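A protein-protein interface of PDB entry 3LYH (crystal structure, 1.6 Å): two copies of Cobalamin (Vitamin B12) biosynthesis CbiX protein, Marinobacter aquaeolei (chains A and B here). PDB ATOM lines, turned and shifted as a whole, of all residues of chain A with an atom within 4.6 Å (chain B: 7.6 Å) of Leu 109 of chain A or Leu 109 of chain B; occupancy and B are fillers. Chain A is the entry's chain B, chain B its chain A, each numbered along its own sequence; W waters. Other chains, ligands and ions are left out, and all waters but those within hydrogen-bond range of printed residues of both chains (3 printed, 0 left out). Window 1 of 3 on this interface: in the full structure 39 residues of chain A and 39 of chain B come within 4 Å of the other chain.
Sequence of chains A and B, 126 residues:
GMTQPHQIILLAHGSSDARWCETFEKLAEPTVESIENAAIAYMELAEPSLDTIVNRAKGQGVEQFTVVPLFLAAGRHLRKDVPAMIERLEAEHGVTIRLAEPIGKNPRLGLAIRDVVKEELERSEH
The side-chain carboxylate of Asp 115 of chain B lies within salt-bridge range of the guanidinium group of Arg 108 of chain A, at 3.7 Å.
The backbone carbonyl oxygen (O) of Phe 71 of chain B lies within hydrogen-bond range of the backbone NH (N) of Gly 104 of chain B (3.0 Å). The side-chain amide oxygen (OD1) of Asn 106 of chain B lies within hydrogen-bond range of the backbone NH (N) of Arg 108 of chain B (2.9 Å). The side-chain amide oxygen of Asn 106 of chain A lies within hydrogen-bond range of the backbone NH of Arg 108 of chain A.
Among the printed residues, pairs that only touch across the chains: Leu 27 of chain A with Leu 72 of chain B (3.8 Å), Leu 27 of chain A with Gly 104 of chain B (3.5 Å), Leu 27 of chain A with Leu 109 of chain B (3.6 Å), Leu 27 of chain A with Gly 110 of chain B (3.5 Å), Leu 27 of chain A with Ile 113 of chain B (3.8 Å), Ile 103 of chain A with Ile 113 of chain B (3.8 Å), Asn 106 of chain A with Val 116 of chain B (3.5 Å), Arg 108 of chain A with Val 116 of chain B (3.96 Å), Leu 109 of chain A with Leu 27 of chain B (3.8 Å), Leu 109 of chain A with Leu 109 of chain B (3.0 Å), Leu 109 of chain A with Val 116 of chain B (3.8 Å), Gly 110 of chain A with Leu 27 of chain B (3.4 Å), Gly 110 of chain A with Pro 30 of chain B (3.8 Å), Ala 112 of chain A with Ala 112 of chain B (3.9 Å), Ile 113 of chain A with Leu 27 of chain B (3.9 Å), Ile 113 of chain A with Thr 31 of chain B (3.95 Å), Ile 113 of chain A with Ile 103 of chain B (3.7 Å), Val 116 of chain A with Asn 106 of chain B (3.5 Å) and Val 116 of chain A with Leu 109 of chain B (3.98 Å).
Of the printed residues of chain B, Leu 27 of chain A touches Leu 72 (3.8 Å), Gly 104 (3.5 Å), Leu 109 (3.6 Å), Gly 110 (3.5 Å) and Ile 113 (3.8 Å). Printed residues of chain A within 4 Å of Leu 72 of chain B: Leu 27 (3.8 Å). Printed residues of chain A within 4 Å of Leu 109 of chain B: Leu 27 (3.6 Å), Leu 109 (3.0 Å) and Val 116 (3.98 Å). Of the printed residues of chain A, Asp 115 of chain B touches Arg 108 (3.6 Å). The nearest printed residue of chain B that does not touch Leu 109 of chain A is Ala 112 of chain B (4.3 Å). The nearest printed residue of chain A that does not touch Leu 109 of chain B is Ala 112 of chain A (4.1 Å).
Hydrophobic or aromatic side chains of chain A within 4 Å of the printed part of chain B: Leu 27, Ile 103, Leu 109, Ala 112, Ile 113 and Val 116. Among the printed residues, 20 pairs touch across the chains.
Leu 27 of chain A touches Leu 109 of chain B, and with the chains exchanged Leu 109 of chain A touches Leu 27 of chain B. Asn 106 of chain A touches Val 116 of chain B, and with the chains exchanged Val 116 of chain A touches Asn 106 of chain B. Arg 108 of chain A touches Val 116 of chain B, but with the chains exchanged Val 116 of chain A does not touch Arg 108 of chain B (4.1 Å). Leu 109 of chain B touches its own counterpart, Leu 109 of chain A. Positions printed for both chains: 27, 103, 106, 107, 108, 109, 110, 111, 112, 113 and 116. Of the 20 pairs that touch across the chains among the printed residues, 14 have their exchanged pair printed and touching as well.
Water W1 bridges the side-chain carboxylate of Asp 115 of chain B (2.6 Å) and the guanidinium group of Arg 108 of chain A (3.3 Å). Water W2 lies within hydrogen-bond range of the backbone carbonyl oxygen (O) of Leu 27 of chain B (2.6 Å), the backbone carbonyl oxygen (O) of Gly 110 of chain A (2.7 Å) and the side-chain hydroxyl (OG1) of Thr 31 of chain B (2.8 Å). Water W3 lies within hydrogen-bond range of O of Leu 27 of chain A (2.7 Å) and O of Gly 110 of chain B (2.8 Å).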
ATOM      1  N   LEU A  27      -6.034  -2.277 -11.633  1.00  0.00           N
ATOM      2  CA  LEU A  27      -4.800  -2.708 -12.306  1.00  0.00           C
ATOM      3  C   LEU A  27      -4.506  -4.184 -12.036  1.00  0.00           C
ATOM      4  O   LEU A  27      -4.028  -4.919 -12.921  1.00  0.00           O
ATOM      5  CB  LEU A  27      -3.598  -1.860 -11.882  1.00  0.00           C
ATOM      6  CG  LEU A  27      -3.514  -0.533 -12.641  1.00  0.00           C
ATOM      7  CD1 LEU A  27      -2.559   0.352 -11.889  1.00  0.00           C
ATOM      8  CD2 LEU A  27      -3.036  -0.754 -14.106  1.00  0.00           C
ATOM      9  N   ILE A 103       7.309  -3.842 -12.450  1.00  0.00           N
ATOM     10  CA  ILE A 103       6.677  -3.976 -13.770  1.00  0.00           C
ATOM     11  C   ILE A 103       7.261  -2.985 -14.802  1.00  0.00           C
ATOM     12  O   ILE A 103       7.295  -3.289 -15.977  1.00  0.00           O
ATOM     13  CB  ILE A 103       5.149  -3.924 -13.732  1.00  0.00           C
ATOM     14  CG1 ILE A 103       4.660  -2.577 -13.225  1.00  0.00           C
ATOM     15  CG2 ILE A 103       4.575  -5.141 -12.917  1.00  0.00           C
ATOM     16  CD1 ILE A 103       3.200  -2.394 -13.348  1.00  0.00           C
ATOM     17  N   ASN A 106       9.818  -4.103 -17.420  1.00  0.00           N
ATOM     18  CA  ASN A 106       9.431  -5.083 -18.419  1.00  0.00           C
ATOM     19  C   ASN A 106       9.129  -4.341 -19.713  1.00  0.00           C
ATOM     20  O   ASN A 106       8.381  -3.354 -19.700  1.00  0.00           O
ATOM     21  CB  ASN A 106       8.241  -5.914 -17.933  1.00  0.00           C
ATOM     22  CG  ASN A 106       8.055  -7.182 -18.744  1.00  0.00           C
ATOM     23  OD1 ASN A 106       7.733  -7.111 -19.945  1.00  0.00           O
ATOM     24  ND2 ASN A 106       8.307  -8.321 -18.132  1.00  0.00           N
ATOM     25  N   PRO A 107       9.683  -4.799 -20.855  1.00  0.00           N
ATOM     26  CA  PRO A 107       9.346  -4.177 -22.149  1.00  0.00           C
ATOM     27  C   PRO A 107       7.868  -4.154 -22.480  1.00  0.00           C
ATOM     28  O   PRO A 107       7.433  -3.276 -23.241  1.00  0.00           O
ATOM     29  CB  PRO A 107      10.127  -5.035 -23.162  1.00  0.00           C
ATOM     30  CG  PRO A 107      11.184  -5.667 -22.436  1.00  0.00           C
ATOM     31  CD  PRO A 107      10.777  -5.779 -21.001  1.00  0.00           C
ATOM     32  N   ARG A 108       7.091  -5.084 -21.933  1.00  0.00           N
ATOM     33  CA  ARG A 108       5.663  -5.110 -22.173  1.00  0.00           C
ATOM     34  C   ARG A 108       4.969  -3.815 -21.777  1.00  0.00           C
ATOM     35  O   ARG A 108       3.988  -3.404 -22.404  1.00  0.00           O
ATOM     36  CB  ARG A 108       5.005  -6.294 -21.484  1.00  0.00           C
ATOM     37  CG  ARG A 108       5.398  -7.640 -22.162  1.00  0.00           C
ATOM     38  CD  ARG A 108       4.786  -8.755 -21.333  1.00  0.00           C
ATOM     39  NE  ARG A 108       5.084 -10.057 -21.934  1.00  0.00           N
ATOM     40  CZ  ARG A 108       4.437 -10.574 -22.975  1.00  0.00           C
ATOM     41  NH1 ARG A 108       3.433  -9.930 -23.575  1.00  0.00           N
ATOM     42  NH2 ARG A 108       4.798 -11.767 -23.422  1.00  0.00           N
ATOM     43  N   LEU A 109       5.443  -3.193 -20.700  1.00  0.00           N
ATOM     44  CA  LEU A 109       4.827  -1.912 -20.276  1.00  0.00           C
ATOM     45  C   LEU A 109       5.043  -0.773 -21.274  1.00  0.00           C
ATOM     46  O   LEU A 109       4.110   0.007 -21.535  1.00  0.00           O
ATOM     47  CB  LEU A 109       5.268  -1.518 -18.859  1.00  0.00           C
ATOM     48  CG  LEU A 109       4.429  -2.028 -17.695  1.00  0.00           C
ATOM     49  CD1 LEU A 109       3.069  -1.433 -17.607  1.00  0.00           C
ATOM     50  CD2 LEU A 109       4.287  -3.595 -17.666  1.00  0.00           C
ATOM     51  N   GLY A 110       6.242  -0.645 -21.802  1.00  0.00           N
ATOM     52  CA  GLY A 110       6.505   0.355 -22.844  1.00  0.00           C
ATOM     53  C   GLY A 110       5.620   0.189 -24.084  1.00  0.00           C
ATOM     54  O   GLY A 110       5.144   1.169 -24.675  1.00  0.00           O
ATOM     55  N   LEU A 111       5.339  -1.071 -24.426  1.00  0.00           N
ATOM     56  CA  LEU A 111       4.458  -1.344 -25.544  1.00  0.00           C
ATOM     57  C   LEU A 111       3.013  -0.991 -25.237  1.00  0.00           C
ATOM     58  O   LEU A 111       2.326  -0.373 -26.086  1.00  0.00           O
ATOM     59  CB  LEU A 111       4.569  -2.804 -25.992  1.00  0.00           C
ATOM     60  CG  LEU A 111       5.946  -3.176 -26.523  1.00  0.00           C
ATOM     61  CD1 LEU A 111       5.907  -4.705 -26.699  1.00  0.00           C
ATOM     62  CD2 LEU A 111       6.387  -2.478 -27.766  1.00  0.00           C
ATOM     63  N   ALA A 112       2.560  -1.320 -24.033  1.00  0.00           N
ATOM     64  CA  ALA A 112       1.224  -0.983 -23.576  1.00  0.00           C
ATOM     65  C   ALA A 112       1.060   0.527 -23.580  1.00  0.00           C
ATOM     66  O   ALA A 112       0.054   1.037 -24.026  1.00  0.00           O
ATOM     67  CB  ALA A 112       0.962  -1.515 -22.155  1.00  0.00           C
ATOM     68  N   ILE A 113       2.066   1.236 -23.083  1.00  0.00           N
ATOM     69  CA  ILE A 113       2.029   2.701 -23.065  1.00  0.00           C
ATOM     70  C   ILE A 113       1.885   3.277 -24.477  1.00  0.00           C
ATOM     71  O   ILE A 113       1.085   4.158 -24.739  1.00  0.00           O
ATOM     72  CB  ILE A 113       3.270   3.294 -22.302  1.00  0.00           C
ATOM     73  CG1 ILE A 113       3.159   2.986 -20.820  1.00  0.00           C
ATOM     74  CG2 ILE A 113       3.426   4.787 -22.563  1.00  0.00           C
ATOM     75  CD1 ILE A 113       4.456   3.235 -20.031  1.00  0.00           C
ATOM     76  N   VAL A 116      -1.695   2.870 -25.589  1.00  0.00           N
ATOM     77  CA  VAL A 116      -2.554   3.872 -24.971  1.00  0.00           C
ATOM     78  C   VAL A 116      -2.365   5.224 -25.644  1.00  0.00           C
ATOM     79  O   VAL A 116      -3.343   5.924 -25.933  1.00  0.00           O
ATOM     80  CB  VAL A 116      -2.279   4.005 -23.459  1.00  0.00           C
ATOM     81  CG1 VAL A 116      -3.045   5.174 -22.803  1.00  0.00           C
ATOM     82  CG2 VAL A 116      -2.661   2.689 -22.757  1.00  0.00           C
ATOM     83  N   LYS B  26      13.267   4.522 -21.033  1.00  0.00           N
ATOM     84  CA  LYS B  26      12.991   3.250 -21.688  1.00  0.00           C
ATOM     85  C   LYS B  26      11.486   2.989 -21.806  1.00  0.00           C
ATOM     86  O   LYS B  26      11.018   2.445 -22.827  1.00  0.00           O
ATOM     87  CB  LYS B  26      13.670   2.083 -20.973  1.00  0.00           C
ATOM     88  CG  LYS B  26      15.190   2.058 -21.063  1.00  0.00           C
ATOM     89  CD  LYS B  26      15.723   2.066 -22.485  1.00  0.00           C
ATOM     90  CE  LYS B  26      15.678   0.699 -23.154  1.00  0.00           C
ATOM     91  NZ  LYS B  26      16.102   0.782 -24.594  1.00  0.00           N
ATOM     92  N   LEU B  27      10.709   3.292 -20.776  1.00  0.00           N
ATOM     93  CA  LEU B  27       9.214   3.193 -20.850  1.00  0.00           C
ATOM     94  C   LEU B  27       8.583   4.013 -21.972  1.00  0.00           C
ATOM     95  O   LEU B  27       7.626   3.541 -22.640  1.00  0.00           O
ATOM     96  CB  LEU B  27       8.552   3.608 -19.532  1.00  0.00           C
ATOM     97  CG  LEU B  27       8.587   2.548 -18.418  1.00  0.00           C
ATOM     98  CD1 LEU B  27       8.247   3.178 -17.038  1.00  0.00           C
ATOM     99  CD2 LEU B  27       7.624   1.396 -18.691  1.00  0.00           C
ATOM    100  N   ALA B  28       9.147   5.179 -22.222  1.00  0.00           N
ATOM    101  CA  ALA B  28       8.677   6.086 -23.268  1.00  0.00           C
ATOM    102  C   ALA B  28       9.212   5.707 -24.670  1.00  0.00           C
ATOM    103  O   ALA B  28       8.643   6.161 -25.650  1.00  0.00           O
ATOM    104  CB  ALA B  28       9.093   7.569 -22.988  1.00  0.00           C
ATOM    105  N   PRO B  30       9.283   3.152 -26.888  1.00  0.00           N
ATOM    106  CA  PRO B  30       8.483   2.629 -28.019  1.00  0.00           C
ATOM    107  C   PRO B  30       7.538   3.712 -28.565  1.00  0.00           C
ATOM    108  O   PRO B  30       7.353   3.831 -29.756  1.00  0.00           O
ATOM    109  CB  PRO B  30       7.719   1.438 -27.409  1.00  0.00           C
ATOM    110  CG  PRO B  30       8.596   0.958 -26.369  1.00  0.00           C
ATOM    111  CD  PRO B  30       9.106   2.272 -25.716  1.00  0.00           C
ATOM    112  N   THR B  31       6.955   4.523 -27.683  1.00  0.00           N
ATOM    113  CA  THR B  31       6.192   5.681 -28.127  1.00  0.00           C
ATOM    114  C   THR B  31       7.000   6.724 -28.889  1.00  0.00           C
ATOM    115  O   THR B  31       6.603   7.184 -29.964  1.00  0.00           O
ATOM    116  CB  THR B  31       5.532   6.410 -26.937  1.00  0.00           C
ATOM    117  OG1 THR B  31       4.677   5.512 -26.240  1.00  0.00           O
ATOM    118  CG2 THR B  31       4.699   7.601 -27.428  1.00  0.00           C
ATOM    119  N   PHE B  71       1.526   7.758 -15.049  1.00  0.00           N
ATOM    120  CA  PHE B  71       1.243   7.511 -13.628  1.00  0.00           C
ATOM    121  C   PHE B  71       0.377   6.272 -13.591  1.00  0.00           C
ATOM    122  O   PHE B  71      -0.626   6.203 -14.325  1.00  0.00           O
ATOM    123  CB  PHE B  71       0.347   8.583 -12.949  1.00  0.00           C
ATOM    124  CG  PHE B  71       0.827  10.013 -13.046  1.00  0.00           C
ATOM    125  CD1 PHE B  71       2.164  10.343 -13.144  1.00  0.00           C
ATOM    126  CD2 PHE B  71      -0.117  11.040 -13.020  1.00  0.00           C
ATOM    127  CE1 PHE B  71       2.556  11.686 -13.217  1.00  0.00           C
ATOM    128  CE2 PHE B  71       0.265  12.349 -13.095  1.00  0.00           C
ATOM    129  CZ  PHE B  71       1.588  12.681 -13.188  1.00  0.00           C
ATOM    130  N   LEU B  72       0.696   5.317 -12.715  1.00  0.00           N
ATOM    131  CA  LEU B  72      -0.245   4.232 -12.452  1.00  0.00           C
ATOM    132  C   LEU B  72      -1.493   4.704 -11.722  1.00  0.00           C
ATOM    133  O   LEU B  72      -2.544   4.126 -11.910  1.00  0.00           O
ATOM    134  CB  LEU B  72       0.407   3.055 -11.725  1.00  0.00           C
ATOM    135  CG  LEU B  72       1.548   2.362 -12.500  1.00  0.00           C
ATOM    136  CD1 LEU B  72       2.267   1.289 -11.685  1.00  0.00           C
ATOM    137  CD2 LEU B  72       0.971   1.739 -13.765  1.00  0.00           C
ATOM    138  N   PRO B 102      -4.622   9.290 -16.613  1.00  0.00           N
ATOM    139  CA  PRO B 102      -3.349   8.560 -16.375  1.00  0.00           C
ATOM    140  C   PRO B 102      -3.377   7.157 -16.985  1.00  0.00           C
ATOM    141  O   PRO B 102      -4.431   6.565 -17.096  1.00  0.00           O
ATOM    142  CB  PRO B 102      -3.244   8.492 -14.855  1.00  0.00           C
ATOM    143  CG  PRO B 102      -4.590   8.878 -14.307  1.00  0.00           C
ATOM    144  CD  PRO B 102      -5.374   9.562 -15.363  1.00  0.00           C
ATOM    145  N   ILE B 103      -2.218   6.701 -17.453  1.00  0.00           N
ATOM    146  CA  ILE B 103      -2.154   5.393 -18.076  1.00  0.00           C
ATOM    147  C   ILE B 103      -2.663   4.288 -17.171  1.00  0.00           C
ATOM    148  O   ILE B 103      -3.206   3.293 -17.673  1.00  0.00           O
ATOM    149  CB  ILE B 103      -0.751   5.041 -18.568  1.00  0.00           C
ATOM    150  CG1 ILE B 103       0.251   5.009 -17.392  1.00  0.00           C
ATOM    151  CG2 ILE B 103      -0.278   5.988 -19.678  1.00  0.00           C
ATOM    152  CD1 ILE B 103       1.528   4.312 -17.736  1.00  0.00           C
ATOM    153  N   GLY B 104      -2.518   4.450 -15.863  1.00  0.00           N
ATOM    154  CA  GLY B 104      -3.056   3.427 -14.949  1.00  0.00           C
ATOM    155  C   GLY B 104      -4.556   3.185 -14.984  1.00  0.00           C
ATOM    156  O   GLY B 104      -5.025   2.144 -14.499  1.00  0.00           O
ATOM    157  N   LYS B 105      -5.315   4.133 -15.533  1.00  0.00           N
ATOM    158  CA  LYS B 105      -6.752   3.951 -15.705  1.00  0.00           C
ATOM    159  C   LYS B 105      -7.124   3.139 -16.926  1.00  0.00           C
ATOM    160  O   LYS B 105      -8.290   2.752 -17.070  1.00  0.00           O
ATOM    161  CB  LYS B 105      -7.502   5.316 -15.720  1.00  0.00           C
ATOM    162  CG  LYS B 105      -7.555   5.990 -14.344  1.00  0.00           C
ATOM    163  CD  LYS B 105      -8.640   7.114 -14.369  1.00  0.00           C
ATOM    164  CE  LYS B 105      -9.036   7.615 -12.973  1.00  0.00           C
ATOM    165  NZ  LYS B 105     -10.289   8.470 -13.003  1.00  0.00           N
ATOM    166  N   ASN B 106      -6.178   2.904 -17.823  1.00  0.00           N
ATOM    167  CA  ASN B 106      -6.477   2.220 -19.080  1.00  0.00           C
ATOM    168  C   ASN B 106      -6.389   0.724 -18.866  1.00  0.00           C
ATOM    169  O   ASN B 106      -5.396   0.228 -18.352  1.00  0.00           O
ATOM    170  CB  ASN B 106      -5.522   2.657 -20.161  1.00  0.00           C
ATOM    171  CG  ASN B 106      -5.963   2.287 -21.550  1.00  0.00           C
ATOM    172  OD1 ASN B 106      -5.918   1.104 -21.953  1.00  0.00           O
ATOM    173  ND2 ASN B 106      -6.275   3.302 -22.349  1.00  0.00           N
ATOM    174  N   PRO B 107      -7.423  -0.004 -19.340  1.00  0.00           N
ATOM    175  CA  PRO B 107      -7.444  -1.454 -19.204  1.00  0.00           C
ATOM    176  C   PRO B 107      -6.247  -2.166 -19.844  1.00  0.00           C
ATOM    177  O   PRO B 107      -5.875  -3.225 -19.371  1.00  0.00           O
ATOM    178  CB  PRO B 107      -8.755  -1.859 -19.907  1.00  0.00           C
ATOM    179  CG  PRO B 107      -9.356  -0.674 -20.411  1.00  0.00           C
ATOM    180  CD  PRO B 107      -8.648   0.526 -19.954  1.00  0.00           C
ATOM    181  N   ARG B 108      -5.595  -1.578 -20.854  1.00  0.00           N
ATOM    182  CA  ARG B 108      -4.408  -2.183 -21.415  1.00  0.00           C
ATOM    183  C   ARG B 108      -3.300  -2.410 -20.413  1.00  0.00           C
ATOM    184  O   ARG B 108      -2.506  -3.329 -20.576  1.00  0.00           O
ATOM    185  CB  ARG B 108      -3.831  -1.366 -22.568  1.00  0.00           C
ATOM    186  CG  ARG B 108      -4.740  -1.397 -23.783  1.00  0.00           C
ATOM    187  CD  ARG B 108      -4.306  -0.406 -24.820  1.00  0.00           C
ATOM    188  NE  ARG B 108      -5.196  -0.552 -25.974  1.00  0.00           N
ATOM    189  CZ  ARG B 108      -5.121  -1.519 -26.884  1.00  0.00           C
ATOM    190  NH1 ARG B 108      -4.158  -2.434 -26.862  1.00  0.00           N
ATOM    191  NH2 ARG B 108      -6.028  -1.556 -27.858  1.00  0.00           N
ATOM    192  N   LEU B 109      -3.222  -1.571 -19.368  1.00  0.00           N
ATOM    193  CA  LEU B 109      -2.156  -1.721 -18.379  1.00  0.00           C
ATOM    194  C   LEU B 109      -2.432  -2.956 -17.494  1.00  0.00           C
ATOM    195  O   LEU B 109      -1.514  -3.665 -17.159  1.00  0.00           O
ATOM    196  CB  LEU B 109      -1.945  -0.437 -17.558  1.00  0.00           C
ATOM    197  CG  LEU B 109      -0.893   0.551 -18.093  1.00  0.00           C
ATOM    198  CD1 LEU B 109       0.511   0.024 -17.918  1.00  0.00           C
ATOM    199  CD2 LEU B 109      -1.133   0.882 -19.553  1.00  0.00           C
ATOM    200  N   GLY B 110      -3.699  -3.186 -17.131  1.00  0.00           N
ATOM    201  CA  GLY B 110      -4.058  -4.364 -16.387  1.00  0.00           C
ATOM    202  C   GLY B 110      -3.726  -5.638 -17.146  1.00  0.00           C
ATOM    203  O   GLY B 110      -3.261  -6.624 -16.585  1.00  0.00           O
ATOM    204  N   LEU B 111      -4.005  -5.611 -18.446  1.00  0.00           N
ATOM    205  CA  LEU B 111      -3.666  -6.751 -19.297  1.00  0.00           C
ATOM    206  C   LEU B 111      -2.142  -6.983 -19.423  1.00  0.00           C
ATOM    207  O   LEU B 111      -1.655  -8.121 -19.370  1.00  0.00           O
ATOM    208  CB  LEU B 111      -4.323  -6.603 -20.693  1.00  0.00           C
ATOM    209  CG  LEU B 111      -5.832  -6.413 -20.676  1.00  0.00           C
ATOM    210  CD1 LEU B 111      -6.376  -6.230 -22.142  1.00  0.00           C
ATOM    211  CD2 LEU B 111      -6.555  -7.567 -19.978  1.00  0.00           C
ATOM    212  N   ALA B 112      -1.371  -5.908 -19.567  1.00  0.00           N
ATOM    213  CA  ALA B 112       0.072  -6.010 -19.601  1.00  0.00           C
ATOM    214  C   ALA B 112       0.613  -6.616 -18.295  1.00  0.00           C
ATOM    215  O   ALA B 112       1.520  -7.459 -18.306  1.00  0.00           O
ATOM    216  CB  ALA B 112       0.687  -4.614 -19.863  1.00  0.00           C
ATOM    217  N   ILE B 113       0.067  -6.171 -17.164  1.00  0.00           N
ATOM    218  CA  ILE B 113       0.490  -6.690 -15.871  1.00  0.00           C
ATOM    219  C   ILE B 113       0.283  -8.219 -15.811  1.00  0.00           C
ATOM    220  O   ILE B 113       1.154  -8.965 -15.354  1.00  0.00           O
ATOM    221  CB  ILE B 113      -0.214  -5.948 -14.702  1.00  0.00           C
ATOM    222  CG1 ILE B 113       0.331  -4.519 -14.601  1.00  0.00           C
ATOM    223  CG2 ILE B 113       0.046  -6.654 -13.382  1.00  0.00           C
ATOM    224  CD1 ILE B 113      -0.548  -3.569 -13.822  1.00  0.00           C
ATOM    225  N   ARG B 114      -0.889  -8.694 -16.228  1.00  0.00           N
ATOM    226  CA  ARG B 114      -1.119 -10.138 -16.311  1.00  0.00           C
ATOM    227  C   ARG B 114      -0.071 -10.867 -17.170  1.00  0.00           C
ATOM    228  O   ARG B 114       0.445 -11.885 -16.734  1.00  0.00           O
ATOM    229  CB  ARG B 114      -2.516 -10.426 -16.840  1.00  0.00           C
ATOM    230  CG  ARG B 114      -2.834 -11.891 -16.791  1.00  0.00           C
ATOM    231  CD  ARG B 114      -4.150 -12.257 -17.317  1.00  0.00           C
ATOM    232  NE  ARG B 114      -4.290 -11.790 -18.691  1.00  0.00           N
ATOM    233  CZ  ARG B 114      -5.436 -11.433 -19.263  1.00  0.00           C
ATOM    234  NH1 ARG B 114      -6.587 -11.432 -18.589  1.00  0.00           N
ATOM    235  NH2 ARG B 114      -5.414 -11.028 -20.528  1.00  0.00           N
ATOM    236  N   ASP B 115       0.283 -10.297 -18.329  1.00  0.00           N
ATOM    237  CA  ASP B 115       1.325 -10.869 -19.190  1.00  0.00           C
ATOM    238  C   ASP B 115       2.675 -10.928 -18.487  1.00  0.00           C
ATOM    239  O   ASP B 115       3.440 -11.910 -18.613  1.00  0.00           O
ATOM    240  CB  ASP B 115       1.475 -10.081 -20.520  1.00  0.00           C
ATOM    241  CG  ASP B 115       0.219 -10.125 -21.422  1.00  0.00           C
ATOM    242  OD1 ASP B 115      -0.598 -11.055 -21.296  1.00  0.00           O
ATOM    243  OD2 ASP B 115       0.054  -9.190 -22.264  1.00  0.00           O
ATOM    244  N   VAL B 116       3.006  -9.874 -17.737  1.00  0.00           N
ATOM    245  CA  VAL B 116       4.240  -9.843 -17.003  1.00  0.00           C
ATOM    246  C   VAL B 116       4.241 -10.902 -15.899  1.00  0.00           C
ATOM    247  O   VAL B 116       5.255 -11.582 -15.664  1.00  0.00           O
ATOM    248  CB  VAL B 116       4.513  -8.423 -16.431  1.00  0.00           C
ATOM    249  CG1 VAL B 116       5.685  -8.448 -15.491  1.00  0.00           C
ATOM    250  CG2 VAL B 116       4.778  -7.411 -17.611  1.00  0.00           C
HETATM  251  O   HOH W   1       1.761  -7.308 -22.595  1.00  0.00           O
HETATM  252  O   HOH W   2       6.201   3.668 -24.840  1.00  0.00           O
HETATM  253  O   HOH W   3      -3.581  -7.368 -13.890  1.00  0.00           O
